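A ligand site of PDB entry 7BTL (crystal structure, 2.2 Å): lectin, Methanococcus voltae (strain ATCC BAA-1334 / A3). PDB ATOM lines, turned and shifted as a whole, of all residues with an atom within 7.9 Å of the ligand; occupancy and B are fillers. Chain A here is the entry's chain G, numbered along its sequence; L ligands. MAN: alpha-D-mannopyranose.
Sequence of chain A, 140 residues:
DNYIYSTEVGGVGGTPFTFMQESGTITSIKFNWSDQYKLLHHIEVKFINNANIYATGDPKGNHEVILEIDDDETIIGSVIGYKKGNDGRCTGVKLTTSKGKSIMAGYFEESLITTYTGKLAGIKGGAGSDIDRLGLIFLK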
ATOM      1  N   GLY A  13      -4.938   4.828 -19.325  1.00  0.00           N
ATOM      2  CA  GLY A  13      -5.868   4.857 -20.479  1.00  0.00           C
ATOM      3  C   GLY A  13      -5.488   3.920 -21.674  1.00  0.00           C
ATOM      4  O   GLY A  13      -5.124   4.430 -22.781  1.00  0.00           O
ATOM      5  N   GLY A  14      -5.642   2.590 -21.541  1.00  0.00           N
ATOM      6  CA  GLY A  14      -5.211   1.605 -22.553  1.00  0.00           C
ATOM      7  C   GLY A  14      -5.802   0.230 -22.391  1.00  0.00           C
ATOM      8  O   GLY A  14      -6.938   0.094 -22.704  1.00  0.00           O
ATOM      9  N   THR A  15      -4.968  -0.797 -22.124  1.00  0.00           N
ATOM     10  CA  THR A  15      -5.299  -2.188 -21.759  1.00  0.00           C
ATOM     11  C   THR A  15      -4.005  -2.880 -21.306  1.00  0.00           C
ATOM     12  O   THR A  15      -3.074  -2.979 -22.102  1.00  0.00           O
ATOM     13  CB  THR A  15      -5.884  -3.001 -22.939  1.00  0.00           C
ATOM     14  OG1 THR A  15      -7.172  -2.508 -23.323  1.00  0.00           O
ATOM     15  CG2 THR A  15      -5.947  -4.490 -22.644  1.00  0.00           C
ATOM     16  N   LEU A  39       3.824  10.207 -30.523  1.00  0.00           N
ATOM     17  CA  LEU A  39       3.563   9.136 -29.540  1.00  0.00           C
ATOM     18  C   LEU A  39       4.239   7.861 -29.981  1.00  0.00           C
ATOM     19  O   LEU A  39       4.334   7.662 -31.179  1.00  0.00           O
ATOM     20  CB  LEU A  39       2.046   8.889 -29.489  1.00  0.00           C
ATOM     21  CG  LEU A  39       1.194  10.039 -28.992  1.00  0.00           C
ATOM     22  CD1 LEU A  39      -0.236   9.555 -28.804  1.00  0.00           C
ATOM     23  CD2 LEU A  39       1.737  10.615 -27.708  1.00  0.00           C
ATOM     24  N   LEU A  40       4.530   6.985 -29.028  1.00  0.00           N
ATOM     25  CA  LEU A  40       4.670   5.546 -29.290  1.00  0.00           C
ATOM     26  C   LEU A  40       3.266   4.947 -29.458  1.00  0.00           C
ATOM     27  O   LEU A  40       2.367   5.294 -28.659  1.00  0.00           O
ATOM     28  CB  LEU A  40       5.397   4.869 -28.122  1.00  0.00           C
ATOM     29  CG  LEU A  40       6.774   5.418 -27.736  1.00  0.00           C
ATOM     30  CD1 LEU A  40       7.365   4.551 -26.666  1.00  0.00           C
ATOM     31  CD2 LEU A  40       7.747   5.480 -28.889  1.00  0.00           C
ATOM     32  N   HIS A  41       3.123   4.027 -30.406  1.00  0.00           N
ATOM     33  CA  HIS A  41       1.821   3.409 -30.804  1.00  0.00           C
ATOM     34  C   HIS A  41       1.914   1.904 -30.607  1.00  0.00           C
ATOM     35  O   HIS A  41       0.924   1.288 -30.262  1.00  0.00           O
ATOM     36  CB  HIS A  41       1.455   3.727 -32.248  1.00  0.00           C
ATOM     37  CG  HIS A  41       1.178   5.152 -32.499  1.00  0.00           C
ATOM     38  ND1 HIS A  41       0.100   5.779 -31.905  1.00  0.00           N
ATOM     39  CD2 HIS A  41       1.821   6.060 -33.289  1.00  0.00           C
ATOM     40  CE1 HIS A  41       0.068   7.051 -32.299  1.00  0.00           C
ATOM     41  NE2 HIS A  41       1.115   7.253 -33.160  1.00  0.00           N
ATOM     42  N   GLY A  57      -0.475  -2.663 -28.988  1.00  0.00           N
ATOM     43  CA  GLY A  57      -0.680  -1.338 -29.578  1.00  0.00           C
ATOM     44  C   GLY A  57      -0.925  -1.457 -31.047  1.00  0.00           C
ATOM     45  O   GLY A  57      -0.775  -2.526 -31.572  1.00  0.00           O
ATOM     46  N   ASP A  58      -1.305  -0.353 -31.660  1.00  0.00           N
ATOM     47  CA  ASP A  58      -1.709  -0.243 -33.082  1.00  0.00           C
ATOM     48  C   ASP A  58      -0.511   0.215 -33.886  1.00  0.00           C
ATOM     49  O   ASP A  58      -0.070   1.328 -33.709  1.00  0.00           O
ATOM     50  CB  ASP A  58      -2.926   0.687 -33.148  1.00  0.00           C
ATOM     51  CG  ASP A  58      -3.662   0.732 -34.473  1.00  0.00           C
ATOM     52  OD1 ASP A  58      -3.105   0.352 -35.524  1.00  0.00           O
ATOM     53  OD2 ASP A  58      -4.890   1.034 -34.422  1.00  0.00           O
ATOM     54  N   LYS A  60       0.423   1.981 -36.282  1.00  0.00           N
ATOM     55  CA  LYS A  60      -0.057   3.037 -37.209  1.00  0.00           C
ATOM     56  C   LYS A  60       0.967   4.144 -37.405  1.00  0.00           C
ATOM     57  O   LYS A  60       0.705   5.049 -38.180  1.00  0.00           O
ATOM     58  CB  LYS A  60      -1.380   3.618 -36.659  1.00  0.00           C
ATOM     59  CG  LYS A  60      -1.260   4.412 -35.363  1.00  0.00           C
ATOM     60  CD  LYS A  60      -2.571   4.569 -34.588  1.00  0.00           C
ATOM     61  CE  LYS A  60      -3.162   5.949 -34.708  1.00  0.00           C
ATOM     62  NZ  LYS A  60      -4.382   6.063 -33.883  1.00  0.00           N
ATOM     63  N   ASP A  87      -4.468  10.480 -18.149  1.00  0.00           N
ATOM     64  CA  ASP A  87      -4.659  10.398 -19.618  1.00  0.00           C
ATOM     65  C   ASP A  87      -3.279  10.535 -20.259  1.00  0.00           C
ATOM     66  O   ASP A  87      -3.188  11.103 -21.333  1.00  0.00           O
ATOM     67  CB  ASP A  87      -5.566  11.483 -20.194  1.00  0.00           C
ATOM     68  CG  ASP A  87      -6.001  11.141 -21.614  1.00  0.00           C
ATOM     69  OD1 ASP A  87      -6.273   9.949 -21.893  1.00  0.00           O
ATOM     70  OD2 ASP A  87      -6.068  12.066 -22.457  1.00  0.00           O
ATOM     71  N   GLY A  88      -2.257  10.028 -19.588  1.00  0.00           N
ATOM     72  CA  GLY A  88      -0.868  10.083 -20.093  1.00  0.00           C
ATOM     73  C   GLY A  88      -0.604   9.064 -21.211  1.00  0.00           C
ATOM     74  O   GLY A  88      -1.456   8.171 -21.406  1.00  0.00           O
ATOM     75  N   ARG A  89       0.519   9.255 -21.920  1.00  0.00           N
ATOM     76  CA  ARG A  89       1.017   8.460 -23.069  1.00  0.00           C
ATOM     77  C   ARG A  89       2.562   8.358 -23.005  1.00  0.00           C
ATOM     78  O   ARG A  89       3.186   9.298 -22.450  1.00  0.00           O
ATOM     79  CB  ARG A  89       0.600   9.181 -24.342  1.00  0.00           C
ATOM     80  N   GLY A 126       0.286  -0.567 -20.539  1.00  0.00           N
ATOM     81  CA  GLY A 126      -1.026  -0.589 -21.181  1.00  0.00           C
ATOM     82  C   GLY A 126      -0.917   0.045 -22.541  1.00  0.00           C
ATOM     83  O   GLY A 126      -0.145   1.018 -22.676  1.00  0.00           O
ATOM     84  N   ALA A 127      -1.649  -0.516 -23.512  1.00  0.00           N
ATOM     85  CA  ALA A 127      -1.718  -0.004 -24.892  1.00  0.00           C
ATOM     86  C   ALA A 127      -3.108  -0.271 -25.484  1.00  0.00           C
ATOM     87  O   ALA A 127      -3.774  -1.286 -25.091  1.00  0.00           O
ATOM     88  CB  ALA A 127      -0.615  -0.631 -25.694  1.00  0.00           C
ATOM     89  N   GLY A 128      -3.521   0.649 -26.332  1.00  0.00           N
ATOM     90  CA  GLY A 128      -4.655   0.489 -27.229  1.00  0.00           C
ATOM     91  C   GLY A 128      -4.281   1.014 -28.589  1.00  0.00           C
ATOM     92  O   GLY A 128      -3.523   0.259 -29.311  1.00  0.00           O
ATOM     93  N   SER A 129      -4.713   2.242 -28.928  1.00  0.00           N
ATOM     94  CA  SER A 129      -4.290   2.900 -30.185  1.00  0.00           C
ATOM     95  C   SER A 129      -2.832   3.394 -30.022  1.00  0.00           C
ATOM     96  O   SER A 129      -2.117   3.639 -31.075  1.00  0.00           O
ATOM     97  CB  SER A 129      -5.179   4.000 -30.536  1.00  0.00           C
ATOM     98  OG  SER A 129      -4.978   4.317 -31.901  1.00  0.00           O
ATOM     99  N   ASP A 130      -2.423   3.571 -28.755  1.00  0.00           N
ATOM    100  CA  ASP A 130      -1.147   4.218 -28.369  1.00  0.00           C
ATOM    101  C   ASP A 130      -0.512   3.316 -27.313  1.00  0.00           C
ATOM    102  O   ASP A 130      -1.174   2.340 -26.826  1.00  0.00           O
ATOM    103  CB  ASP A 130      -1.414   5.626 -27.864  1.00  0.00           C
ATOM    104  CG  ASP A 130      -2.144   6.536 -28.831  1.00  0.00           C
ATOM    105  OD1 ASP A 130      -2.089   6.296 -30.088  1.00  0.00           O
ATOM    106  OD2 ASP A 130      -2.817   7.484 -28.301  1.00  0.00           O
ATOM    107  N   ILE A 131       0.748   3.568 -26.978  1.00  0.00           N
ATOM    108  CA  ILE A 131       1.325   3.048 -25.715  1.00  0.00           C
ATOM    109  C   ILE A 131       0.911   4.051 -24.612  1.00  0.00           C
ATOM    110  O   ILE A 131       1.512   5.136 -24.557  1.00  0.00           O
ATOM    111  CB  ILE A 131       2.838   2.866 -25.836  1.00  0.00           C
ATOM    112  CG1 ILE A 131       3.204   2.036 -27.084  1.00  0.00           C
ATOM    113  CG2 ILE A 131       3.382   2.267 -24.553  1.00  0.00           C
ATOM    114  CD1 ILE A 131       2.765   0.591 -27.056  1.00  0.00           C
HETATM  115  C1  MAN L   1      -7.941   3.156 -26.180  1.00  0.00           C
HETATM  116  C2  MAN L   1      -9.050   3.127 -27.177  1.00  0.00           C
HETATM  117  C3  MAN L   1      -8.978   4.248 -28.505  1.00  0.00           C
HETATM  118  C4  MAN L   1      -8.612   5.583 -28.031  1.00  0.00           C
HETATM  119  C5  MAN L   1      -7.310   5.138 -27.145  1.00  0.00           C
HETATM  120  C6  MAN L   1      -6.112   6.035 -26.683  1.00  0.00           C
HETATM  121  O1  MAN L   1      -6.787   2.452 -26.740  1.00  0.00           O
HETATM  122  O2  MAN L   1     -10.126   3.241 -26.255  1.00  0.00           O
HETATM  123  O3  MAN L   1     -10.092   4.417 -29.716  1.00  0.00           O
HETATM  124  O4  MAN L   1      -8.616   6.273 -29.420  1.00  0.00           O
HETATM  125  O5  MAN L   1      -7.785   4.563 -25.838  1.00  0.00           O
HETATM  126  O6  MAN L   1      -5.027   5.793 -27.557  1.00  0.00           O
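Merely in contact with the ligand: Gly 128. Within 4 Å of the ligand: Gly 128, Ser 129 and Asp 130.
An oxygen (O6) of the ligand is in hydrogen-bond range of the side-chain carboxylate (OD2) of Asp 130, 2.9 Å away. O1 of the ligand lies within hydrogen-bond range of N of Ser 129 (3.0 Å).
ND1 of His 41 lies within hydrogen-bond range of OD1 of Asp 130 (2.9 Å). The backbone NH of Asp 58 is in hydrogen-bond range of the backbone carbonyl oxygen of Gly 128 (3.3 Å). OG of Ser 129 sits at hydrogen-bond distance from NZ of Lys 60, 2.7 Å away. ND1 of His 41 lies within hydrogen-bond range of O of Ser 129 (3.2 Å).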
